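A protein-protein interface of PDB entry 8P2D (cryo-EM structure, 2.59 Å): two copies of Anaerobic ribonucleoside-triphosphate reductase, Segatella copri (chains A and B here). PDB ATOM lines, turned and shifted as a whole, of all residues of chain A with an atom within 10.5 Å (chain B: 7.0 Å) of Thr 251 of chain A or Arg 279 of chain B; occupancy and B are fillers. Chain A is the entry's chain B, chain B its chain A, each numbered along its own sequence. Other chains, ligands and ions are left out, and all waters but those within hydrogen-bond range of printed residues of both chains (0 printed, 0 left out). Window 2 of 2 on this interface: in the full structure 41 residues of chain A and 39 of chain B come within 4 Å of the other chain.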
ATOM      1  N   VAL A 244     -16.228  -3.379  27.576  1.00  0.00           N
ATOM      2  CA  VAL A 244     -17.527  -2.857  27.990  1.00  0.00           C
ATOM      3  C   VAL A 244     -18.243  -2.213  26.813  1.00  0.00           C
ATOM      4  O   VAL A 244     -19.463  -2.354  26.654  1.00  0.00           O
ATOM      5  CB  VAL A 244     -17.358  -1.876  29.167  1.00  0.00           C
ATOM      6  CG1 VAL A 244     -18.547  -0.933  29.260  1.00  0.00           C
ATOM      7  CG2 VAL A 244     -17.196  -2.641  30.469  1.00  0.00           C
ATOM      8  N   LYS A 245     -17.499  -1.521  25.954  1.00  0.00           N
ATOM      9  CA  LYS A 245     -18.088  -0.892  24.780  1.00  0.00           C
ATOM     10  C   LYS A 245     -18.188  -1.844  23.588  1.00  0.00           C
ATOM     11  O   LYS A 245     -18.263  -1.385  22.443  1.00  0.00           O
ATOM     12  CB  LYS A 245     -17.301   0.364  24.404  1.00  0.00           C
ATOM     13  CG  LYS A 245     -17.946   1.650  24.904  1.00  0.00           C
ATOM     14  CD  LYS A 245     -18.315   1.550  26.379  1.00  0.00           C
ATOM     15  CE  LYS A 245     -19.784   1.869  26.611  1.00  0.00           C
ATOM     16  NZ  LYS A 245     -20.163   1.709  28.042  1.00  0.00           N
ATOM     17  N   ASN A 246     -18.199  -3.156  23.834  1.00  0.00           N
ATOM     18  CA  ASN A 246     -18.358  -4.151  22.785  1.00  0.00           C
ATOM     19  C   ASN A 246     -19.544  -5.080  22.994  1.00  0.00           C
ATOM     20  O   ASN A 246     -20.015  -5.677  22.019  1.00  0.00           O
ATOM     21  CB  ASN A 246     -17.089  -5.009  22.653  1.00  0.00           C
ATOM     22  CG  ASN A 246     -15.928  -4.249  22.053  1.00  0.00           C
ATOM     23  OD1 ASN A 246     -15.952  -3.022  21.963  1.00  0.00           O
ATOM     24  ND2 ASN A 246     -14.898  -4.977  21.639  1.00  0.00           N
ATOM     25  N   LEU A 247     -20.039  -5.225  24.220  1.00  0.00           N
ATOM     26  CA  LEU A 247     -21.123  -6.156  24.500  1.00  0.00           C
ATOM     27  C   LEU A 247     -22.486  -5.616  24.090  1.00  0.00           C
ATOM     28  O   LEU A 247     -23.447  -6.390  24.016  1.00  0.00           O
ATOM     29  CB  LEU A 247     -21.130  -6.515  25.990  1.00  0.00           C
ATOM     30  CG  LEU A 247     -21.871  -7.783  26.414  1.00  0.00           C
ATOM     31  CD1 LEU A 247     -21.538  -8.935  25.482  1.00  0.00           C
ATOM     32  CD2 LEU A 247     -21.505  -8.136  27.841  1.00  0.00           C
ATOM     33  N   GLU A 248     -22.590  -4.316  23.818  1.00  0.00           N
ATOM     34  CA  GLU A 248     -23.828  -3.727  23.331  1.00  0.00           C
ATOM     35  C   GLU A 248     -24.052  -3.967  21.845  1.00  0.00           C
ATOM     36  O   GLU A 248     -25.141  -3.678  21.344  1.00  0.00           O
ATOM     37  CB  GLU A 248     -23.835  -2.224  23.619  1.00  0.00           C
ATOM     38  CG  GLU A 248     -22.595  -1.498  23.123  1.00  0.00           C
ATOM     39  CD  GLU A 248     -22.664  -0.004  23.354  1.00  0.00           C
ATOM     40  OE1 GLU A 248     -23.665   0.462  23.935  1.00  0.00           O
ATOM     41  OE2 GLU A 248     -21.717   0.704  22.953  1.00  0.00           O
ATOM     42  N   LYS A 249     -23.050  -4.482  21.130  1.00  0.00           N
ATOM     43  CA  LYS A 249     -23.207  -4.709  19.700  1.00  0.00           C
ATOM     44  C   LYS A 249     -24.207  -5.822  19.414  1.00  0.00           C
ATOM     45  O   LYS A 249     -24.866  -5.804  18.368  1.00  0.00           O
ATOM     46  CB  LYS A 249     -21.852  -5.020  19.070  1.00  0.00           C
ATOM     47  CG  LYS A 249     -20.863  -3.869  19.168  1.00  0.00           C
ATOM     48  CD  LYS A 249     -19.513  -4.234  18.569  1.00  0.00           C
ATOM     49  CE  LYS A 249     -18.529  -3.081  18.698  1.00  0.00           C
ATOM     50  NZ  LYS A 249     -17.192  -3.414  18.134  1.00  0.00           N
ATOM     51  N   LEU A 250     -24.333  -6.794  20.317  1.00  0.00           N
ATOM     52  CA  LEU A 250     -25.366  -7.810  20.161  1.00  0.00           C
ATOM     53  C   LEU A 250     -26.751  -7.218  20.390  1.00  0.00           C
ATOM     54  O   LEU A 250     -27.670  -7.437  19.593  1.00  0.00           O
ATOM     55  CB  LEU A 250     -25.109  -8.970  21.122  1.00  0.00           C
ATOM     56  CG  LEU A 250     -26.148 -10.092  21.140  1.00  0.00           C
ATOM     57  CD1 LEU A 250     -26.161 -10.831  19.817  1.00  0.00           C
ATOM     58  CD2 LEU A 250     -25.884 -11.051  22.289  1.00  0.00           C
ATOM     59  N   THR A 251     -26.915  -6.456  21.473  1.00  0.00           N
ATOM     60  CA  THR A 251     -28.178  -5.785  21.794  1.00  0.00           C
ATOM     61  C   THR A 251     -27.831  -4.407  22.349  1.00  0.00           C
ATOM     62  O   THR A 251     -27.351  -4.294  23.482  1.00  0.00           O
ATOM     63  CB  THR A 251     -29.009  -6.588  22.791  1.00  0.00           C
ATOM     64  OG1 THR A 251     -28.176  -7.013  23.878  1.00  0.00           O
ATOM     65  CG2 THR A 251     -29.637  -7.804  22.126  1.00  0.00           C
ATOM     66  N   GLY A 252     -28.066  -3.369  21.549  1.00  0.00           N
ATOM     67  CA  GLY A 252     -27.731  -2.010  21.934  1.00  0.00           C
ATOM     68  C   GLY A 252     -28.408  -1.544  23.207  1.00  0.00           C
ATOM     69  O   GLY A 252     -29.624  -1.692  23.364  1.00  0.00           O
ATOM     70  N   GLU A 253     -27.627  -0.981  24.125  1.00  0.00           N
ATOM     71  CA  GLU A 253     -28.154  -0.487  25.388  1.00  0.00           C
ATOM     72  C   GLU A 253     -27.253   0.631  25.892  1.00  0.00           C
ATOM     73  O   GLU A 253     -26.044   0.630  25.647  1.00  0.00           O
ATOM     74  CB  GLU A 253     -28.261  -1.611  26.427  1.00  0.00           C
ATOM     75  CG  GLU A 253     -29.092  -1.259  27.648  1.00  0.00           C
ATOM     76  CD  GLU A 253     -29.404  -2.470  28.506  1.00  0.00           C
ATOM     77  OE1 GLU A 253     -29.003  -3.589  28.125  1.00  0.00           O
ATOM     78  OE2 GLU A 253     -30.052  -2.302  29.560  1.00  0.00           O
ATOM     79  N   ASP A 254     -27.856   1.588  26.598  1.00  0.00           N
ATOM     80  CA  ASP A 254     -27.138   2.775  27.066  1.00  0.00           C
ATOM     81  C   ASP A 254     -26.491   2.491  28.423  1.00  0.00           C
ATOM     82  O   ASP A 254     -26.912   2.976  29.475  1.00  0.00           O
ATOM     83  CB  ASP A 254     -28.080   3.972  27.130  1.00  0.00           C
ATOM     84  CG  ASP A 254     -27.352   5.274  27.409  1.00  0.00           C
ATOM     85  OD1 ASP A 254     -26.103   5.280  27.393  1.00  0.00           O
ATOM     86  OD2 ASP A 254     -28.032   6.295  27.646  1.00  0.00           O
ATOM     87  N   LEU A 255     -25.436   1.677  28.377  1.00  0.00           N
ATOM     88  CA  LEU A 255     -24.615   1.394  29.554  1.00  0.00           C
ATOM     89  C   LEU A 255     -23.297   2.150  29.407  1.00  0.00           C
ATOM     90  O   LEU A 255     -22.293   1.628  28.924  1.00  0.00           O
ATOM     91  CB  LEU A 255     -24.400  -0.108  29.716  1.00  0.00           C
ATOM     92  CG  LEU A 255     -25.559  -0.881  30.347  1.00  0.00           C
ATOM     93  CD1 LEU A 255     -25.283  -2.376  30.346  1.00  0.00           C
ATOM     94  CD2 LEU A 255     -25.806  -0.381  31.760  1.00  0.00           C
ATOM     95  N   GLY A 276     -30.521 -11.560  33.924  1.00  0.00           N
ATOM     96  CA  GLY A 276     -30.429 -10.130  33.722  1.00  0.00           C
ATOM     97  C   GLY A 276     -29.091  -9.747  33.136  1.00  0.00           C
ATOM     98  O   GLY A 276     -28.318 -10.600  32.693  1.00  0.00           O
ATOM     99  N   ARG A 277     -28.824  -8.439  33.136  1.00  0.00           N
ATOM    100  CA  ARG A 277     -27.529  -7.944  32.688  1.00  0.00           C
ATOM    101  C   ARG A 277     -26.396  -8.375  33.606  1.00  0.00           C
ATOM    102  O   ARG A 277     -25.228  -8.242  33.225  1.00  0.00           O
ATOM    103  CB  ARG A 277     -27.548  -6.419  32.571  1.00  0.00           C
ATOM    104  CG  ARG A 277     -27.767  -5.693  33.884  1.00  0.00           C
ATOM    105  CD  ARG A 277     -29.048  -4.881  33.845  1.00  0.00           C
ATOM    106  NE  ARG A 277     -29.093  -3.999  32.684  1.00  0.00           N
ATOM    107  CZ  ARG A 277     -28.523  -2.804  32.631  1.00  0.00           C
ATOM    108  NH1 ARG A 277     -27.839  -2.318  33.654  1.00  0.00           N
ATOM    109  NH2 ARG A 277     -28.641  -2.079  31.523  1.00  0.00           N
ATOM    110  N   LEU A 280     -24.303 -10.671  31.898  1.00  0.00           N
ATOM    111  CA  LEU A 280     -23.368 -10.082  30.952  1.00  0.00           C
ATOM    112  C   LEU A 280     -22.450  -9.037  31.568  1.00  0.00           C
ATOM    113  O   LEU A 280     -21.364  -8.802  31.029  1.00  0.00           O
ATOM    114  CB  LEU A 280     -24.127  -9.457  29.770  1.00  0.00           C
ATOM    115  CG  LEU A 280     -25.103  -8.302  30.011  1.00  0.00           C
ATOM    116  CD1 LEU A 280     -24.422  -6.944  29.863  1.00  0.00           C
ATOM    117  CD2 LEU A 280     -26.296  -8.409  29.074  1.00  0.00           C
ATOM    118  N   GLU A 281     -22.858  -8.400  32.668  1.00  0.00           N
ATOM    119  CA  GLU A 281     -21.968  -7.463  33.345  1.00  0.00           C
ATOM    120  C   GLU A 281     -20.741  -8.177  33.895  1.00  0.00           C
ATOM    121  O   GLU A 281     -19.617  -7.678  33.773  1.00  0.00           O
ATOM    122  CB  GLU A 281     -22.717  -6.740  34.466  1.00  0.00           C
ATOM    123  CG  GLU A 281     -22.250  -5.315  34.728  1.00  0.00           C
ATOM    124  CD  GLU A 281     -22.878  -4.306  33.783  1.00  0.00           C
ATOM    125  OE1 GLU A 281     -23.429  -4.719  32.742  1.00  0.00           O
ATOM    126  OE2 GLU A 281     -22.831  -3.096  34.086  1.00  0.00           O
ATOM    127  N   LEU B 247     -19.785 -16.296  21.946  1.00  0.00           N
ATOM    128  CA  LEU B 247     -20.918 -15.414  21.722  1.00  0.00           C
ATOM    129  C   LEU B 247     -22.251 -16.054  22.065  1.00  0.00           C
ATOM    130  O   LEU B 247     -23.236 -15.330  22.244  1.00  0.00           O
ATOM    131  CB  LEU B 247     -20.942 -14.940  20.260  1.00  0.00           C
ATOM    132  CG  LEU B 247     -21.739 -13.668  19.960  1.00  0.00           C
ATOM    133  CD1 LEU B 247     -21.490 -12.616  21.029  1.00  0.00           C
ATOM    134  CD2 LEU B 247     -21.370 -13.125  18.591  1.00  0.00           C
ATOM    135  N   LEU B 250     -23.705 -15.501  26.270  1.00  0.00           N
ATOM    136  CA  LEU B 250     -24.779 -14.613  26.698  1.00  0.00           C
ATOM    137  C   LEU B 250     -26.135 -15.129  26.234  1.00  0.00           C
ATOM    138  O   LEU B 250     -27.130 -15.021  26.961  1.00  0.00           O
ATOM    139  CB  LEU B 250     -24.532 -13.199  26.180  1.00  0.00           C
ATOM    140  CG  LEU B 250     -25.615 -12.168  26.497  1.00  0.00           C
ATOM    141  CD1 LEU B 250     -25.872 -12.103  27.994  1.00  0.00           C
ATOM    142  CD2 LEU B 250     -25.225 -10.802  25.958  1.00  0.00           C
ATOM    143  N   THR B 251     -26.196 -15.696  25.032  1.00  0.00           N
ATOM    144  CA  THR B 251     -27.433 -16.222  24.456  1.00  0.00           C
ATOM    145  C   THR B 251     -27.234 -17.714  24.209  1.00  0.00           C
ATOM    146  O   THR B 251     -26.753 -18.118  23.147  1.00  0.00           O
ATOM    147  CB  THR B 251     -27.800 -15.485  23.166  1.00  0.00           C
ATOM    148  OG1 THR B 251     -26.734 -15.617  22.218  1.00  0.00           O
ATOM    149  CG2 THR B 251     -28.044 -14.009  23.446  1.00  0.00           C
ATOM    150  N   LEU B 271     -21.846  -1.934  11.599  1.00  0.00           N
ATOM    151  CA  LEU B 271     -22.865  -2.801  12.185  1.00  0.00           C
ATOM    152  C   LEU B 271     -24.065  -1.933  12.549  1.00  0.00           C
ATOM    153  O   LEU B 271     -24.289  -1.575  13.704  1.00  0.00           O
ATOM    154  CB  LEU B 271     -22.309  -3.547  13.395  1.00  0.00           C
ATOM    155  CG  LEU B 271     -23.195  -4.645  13.988  1.00  0.00           C
ATOM    156  CD1 LEU B 271     -23.415  -5.759  12.976  1.00  0.00           C
ATOM    157  CD2 LEU B 271     -22.591  -5.190  15.270  1.00  0.00           C
ATOM    158  N   GLY B 273     -27.997  -2.168  11.726  1.00  0.00           N
ATOM    159  CA  GLY B 273     -29.178  -2.806  11.180  1.00  0.00           C
ATOM    160  C   GLY B 273     -29.020  -4.289  10.927  1.00  0.00           C
ATOM    161  O   GLY B 273     -28.442  -4.693   9.913  1.00  0.00           O
ATOM    162  N   LEU B 274     -29.537  -5.109  11.840  1.00  0.00           N
ATOM    163  CA  LEU B 274     -29.535  -6.560  11.706  1.00  0.00           C
ATOM    164  C   LEU B 274     -30.416  -7.146  12.799  1.00  0.00           C
ATOM    165  O   LEU B 274     -30.499  -6.599  13.902  1.00  0.00           O
ATOM    166  CB  LEU B 274     -28.117  -7.148  11.794  1.00  0.00           C
ATOM    167  CG  LEU B 274     -27.501  -7.411  13.171  1.00  0.00           C
ATOM    168  CD1 LEU B 274     -26.222  -8.211  13.025  1.00  0.00           C
ATOM    169  CD2 LEU B 274     -27.238  -6.118  13.923  1.00  0.00           C
ATOM    170  N   GLN B 275     -31.062  -8.266  12.484  1.00  0.00           N
ATOM    171  CA  GLN B 275     -31.956  -8.926  13.425  1.00  0.00           C
ATOM    172  C   GLN B 275     -32.018 -10.410  13.104  1.00  0.00           C
ATOM    173  O   GLN B 275     -31.634 -10.849  12.018  1.00  0.00           O
ATOM    174  CB  GLN B 275     -33.366  -8.320  13.395  1.00  0.00           C
ATOM    175  CG  GLN B 275     -33.659  -7.332  14.517  1.00  0.00           C
ATOM    176  CD  GLN B 275     -33.362  -5.896  14.135  1.00  0.00           C
ATOM    177  OE1 GLN B 275     -33.088  -5.593  12.974  1.00  0.00           O
ATOM    178  NE2 GLN B 275     -33.416  -5.001  15.114  1.00  0.00           N
ATOM    179  N   GLY B 276     -32.518 -11.179  14.064  1.00  0.00           N
ATOM    180  CA  GLY B 276     -32.619 -12.616  13.904  1.00  0.00           C
ATOM    181  C   GLY B 276     -31.379 -13.334  14.399  1.00  0.00           C
ATOM    182  O   GLY B 276     -30.635 -12.851  15.258  1.00  0.00           O
ATOM    183  N   ARG B 277     -31.158 -14.523  13.836  1.00  0.00           N
ATOM    184  CA  ARG B 277     -29.975 -15.320  14.157  1.00  0.00           C
ATOM    185  C   ARG B 277     -28.796 -14.892  13.279  1.00  0.00           C
ATOM    186  O   ARG B 277     -28.218 -15.671  12.522  1.00  0.00           O
ATOM    187  CB  ARG B 277     -30.276 -16.806  14.001  1.00  0.00           C
ATOM    188  CG  ARG B 277     -29.223 -17.719  14.610  1.00  0.00           C
ATOM    189  CD  ARG B 277     -29.459 -19.172  14.245  1.00  0.00           C
ATOM    190  NE  ARG B 277     -30.687 -19.694  14.830  1.00  0.00           N
ATOM    191  CZ  ARG B 277     -31.101 -20.948  14.705  1.00  0.00           C
ATOM    192  NH1 ARG B 277     -30.408 -21.839  14.015  1.00  0.00           N
ATOM    193  NH2 ARG B 277     -32.238 -21.318  15.288  1.00  0.00           N
ATOM    194  N   GLU B 278     -28.464 -13.605  13.370  1.00  0.00           N
ATOM    195  CA  GLU B 278     -27.281 -13.078  12.696  1.00  0.00           C
ATOM    196  C   GLU B 278     -26.431 -12.164  13.561  1.00  0.00           C
ATOM    197  O   GLU B 278     -25.243 -12.003  13.262  1.00  0.00           O
ATOM    198  CB  GLU B 278     -27.671 -12.327  11.416  1.00  0.00           C
ATOM    199  CG  GLU B 278     -28.474 -11.060  11.644  1.00  0.00           C
ATOM    200  CD  GLU B 278     -28.753 -10.311  10.354  1.00  0.00           C
ATOM    201  OE1 GLU B 278     -28.010 -10.515   9.372  1.00  0.00           O
ATOM    202  OE2 GLU B 278     -29.719  -9.522  10.319  1.00  0.00           O
ATOM    203  N   ARG B 279     -26.972 -11.561  14.620  1.00  0.00           N
ATOM    204  CA  ARG B 279     -26.146 -10.781  15.530  1.00  0.00           C
ATOM    205  C   ARG B 279     -25.232 -11.654  16.378  1.00  0.00           C
ATOM    206  O   ARG B 279     -24.356 -11.119  17.066  1.00  0.00           O
ATOM    207  CB  ARG B 279     -27.029  -9.910  16.424  1.00  0.00           C
ATOM    208  CG  ARG B 279     -28.336 -10.562  16.836  1.00  0.00           C
ATOM    209  CD  ARG B 279     -29.166  -9.619  17.685  1.00  0.00           C
ATOM    210  NE  ARG B 279     -29.286  -8.303  17.070  1.00  0.00           N
ATOM    211  CZ  ARG B 279     -29.986  -7.299  17.578  1.00  0.00           C
ATOM    212  NH1 ARG B 279     -30.651  -7.425  18.714  1.00  0.00           N
ATOM    213  NH2 ARG B 279     -30.020  -6.138  16.929  1.00  0.00           N
ATOM    214  N   LEU B 280     -25.414 -12.972  16.349  1.00  0.00           N
ATOM    215  CA  LEU B 280     -24.518 -13.911  17.014  1.00  0.00           C
ATOM    216  C   LEU B 280     -23.792 -14.837  16.052  1.00  0.00           C
ATOM    217  O   LEU B 280     -22.654 -15.224  16.322  1.00  0.00           O
ATOM    218  CB  LEU B 280     -25.288 -14.745  18.048  1.00  0.00           C
ATOM    219  CG  LEU B 280     -26.646 -15.356  17.690  1.00  0.00           C
ATOM    220  CD1 LEU B 280     -26.503 -16.710  17.017  1.00  0.00           C
ATOM    221  CD2 LEU B 280     -27.521 -15.466  18.931  1.00  0.00           C
ATOM    222  N   GLU B 281     -24.414 -15.208  14.931  1.00  0.00           N
ATOM    223  CA  GLU B 281     -23.786 -16.108  13.973  1.00  0.00           C
ATOM    224  C   GLU B 281     -23.082 -15.379  12.835  1.00  0.00           C
ATOM    225  O   GLU B 281     -22.279 -15.998  12.130  1.00  0.00           O
ATOM    226  CB  GLU B 281     -24.820 -17.081  13.396  1.00  0.00           C
ATOM    227  CG  GLU B 281     -25.332 -16.709  12.020  1.00  0.00           C
ATOM    228  CD  GLU B 281     -26.211 -17.787  11.418  1.00  0.00           C
ATOM    229  OE1 GLU B 281     -26.223 -18.915  11.954  1.00  0.00           O
ATOM    230  OE2 GLU B 281     -26.892 -17.505  10.409  1.00  0.00           O
ATOM    231  N   GLN B 282     -23.351 -14.090  12.641  1.00  0.00           N
ATOM    232  CA  GLN B 282     -22.681 -13.299  11.617  1.00  0.00           C
ATOM    233  C   GLN B 282     -21.799 -12.204  12.191  1.00  0.00           C
ATOM    234  O   GLN B 282     -20.785 -11.865  11.579  1.00  0.00           O
ATOM    235  CB  GLN B 282     -23.715 -12.679  10.661  1.00  0.00           C
ATOM    236  CG  GLN B 282     -23.132 -11.910   9.483  1.00  0.00           C
ATOM    237  CD  GLN B 282     -22.942 -10.432   9.779  1.00  0.00           C
ATOM    238  OE1 GLN B 282     -23.363  -9.937  10.823  1.00  0.00           O
ATOM    239  NE2 GLN B 282     -22.306  -9.721   8.854  1.00  0.00           N
ATOM    240  N   HIS B 283     -22.153 -11.646  13.349  1.00  0.00           N
ATOM    241  CA  HIS B 283     -21.255 -10.713  14.019  1.00  0.00           C
ATOM    242  C   HIS B 283     -19.997 -11.423  14.502  1.00  0.00           C
ATOM    243  O   HIS B 283     -18.900 -10.854  14.460  1.00  0.00           O
ATOM    244  CB  HIS B 283     -21.977 -10.035  15.181  1.00  0.00           C
ATOM    245  CG  HIS B 283     -21.196  -8.924  15.812  1.00  0.00           C
ATOM    246  ND1 HIS B 283     -21.017  -8.820  17.174  1.00  0.00           N
ATOM    247  CD2 HIS B 283     -20.546  -7.870  15.265  1.00  0.00           C
ATOM    248  CE1 HIS B 283     -20.293  -7.749  17.440  1.00  0.00           C
ATOM    249  NE2 HIS B 283     -19.995  -7.154  16.299  1.00  0.00           N
ATOM    250  N   ALA B 284     -20.140 -12.671  14.961  1.00  0.00           N
ATOM    251  CA  ALA B 284     -18.977 -13.463  15.351  1.00  0.00           C
ATOM    252  C   ALA B 284     -18.034 -13.664  14.173  1.00  0.00           C
ATOM    253  O   ALA B 284     -16.809 -13.621  14.333  1.00  0.00           O
ATOM    254  CB  ALA B 284     -19.422 -14.810  15.917  1.00  0.00           C
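NH1 of Arg 279 of chain B sits close to O of Leu 250 of chain A.
N of His 283 of chain B lies within hydrogen-bond range of O of Glu 278 of chain B, 3.1 Å away.
The backbone carbonyl oxygen (O) of Leu 274 of chain B lies within hydrogen-bond range of the guanidinium group (NH2) of Arg 279 of chain B (3.1 Å).
Among the printed residues, pairs that only touch across the chains: Lys 249 of chain A with His 283 of chain B (3.5 Å), Thr 251 of chain A with Arg 279 of chain B (3.6 Å), Leu 280 of chain A with Leu 250 of chain B (3.6 Å), Leu 250 of chain A with Leu 250 of chain B (3.7 Å), Leu 250 of chain A with Thr 251 of chain B (3.8 Å) and Lys 249 of chain A with Leu 271 of chain B (3.9 Å).
Thr 251 of chain A touches one residue of chain B.
Of chain A, only Leu 250 (3.1 Å) and Thr 251 (3.6 Å) come within 4 Å of Arg 279 of chain B.
Leu 274 of chain B touches none of the printed residues of chain A.
No residue of chain A comes within 4 Å of Gln 275 of chain B.
Glu 278 of chain B touches none of the printed residues of chain A.
No residue of chain A comes within 4 Å of Leu 280 of chain B.
Printed residues of chain B within 4 Å of Lys 249 of chain A: Leu 271 (3.9 Å) and His 283 (3.5 Å).
Of the printed residues of chain A, Leu 271 of chain B touches Lys 249.
Val 244 of chain A touches none of the printed residues of chain B.
The nearest residue of chain B that does not touch Thr 251 of chain A is Leu 250 of chain B (5.2 Å).
The nearest printed residue of chain B that does not touch Leu 250 of chain A is Leu 280 of chain B (4.1 Å).
Of the 16 printed residues of chain B, 5 touch a printed residue of chain A.
Printed residues of chain B that touch a printed residue of chain A: Leu 250, Thr 251, Leu 271, Arg 279 and His 283.
Hydrophobic or aromatic side chains of chain B that line the printed part of chain A: Leu 250, Leu 271 and His 283.
Along chain B the printed residues that touch a printed residue of chain A span positions 250 to 283.
Hydrophobic or aromatic side chains of chain A within 4 Å of the printed part of chain B: Leu 250 and Leu 280.
Leu 250 of chain A touches its own counterpart, Leu 250 of chain B.
Leu 250 of chain A touches Thr 251 of chain B, but with the chains exchanged Thr 251 of chain A does not touch Leu 250 of chain B (5.2 Å).
Leu 280 of chain A touches Leu 250 of chain B, but with the chains exchanged Leu 250 of chain A does not touch Leu 280 of chain B (4.1 Å).
Positions printed for both chains: 247, 250, 251, 276, 277, 280 and 281.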
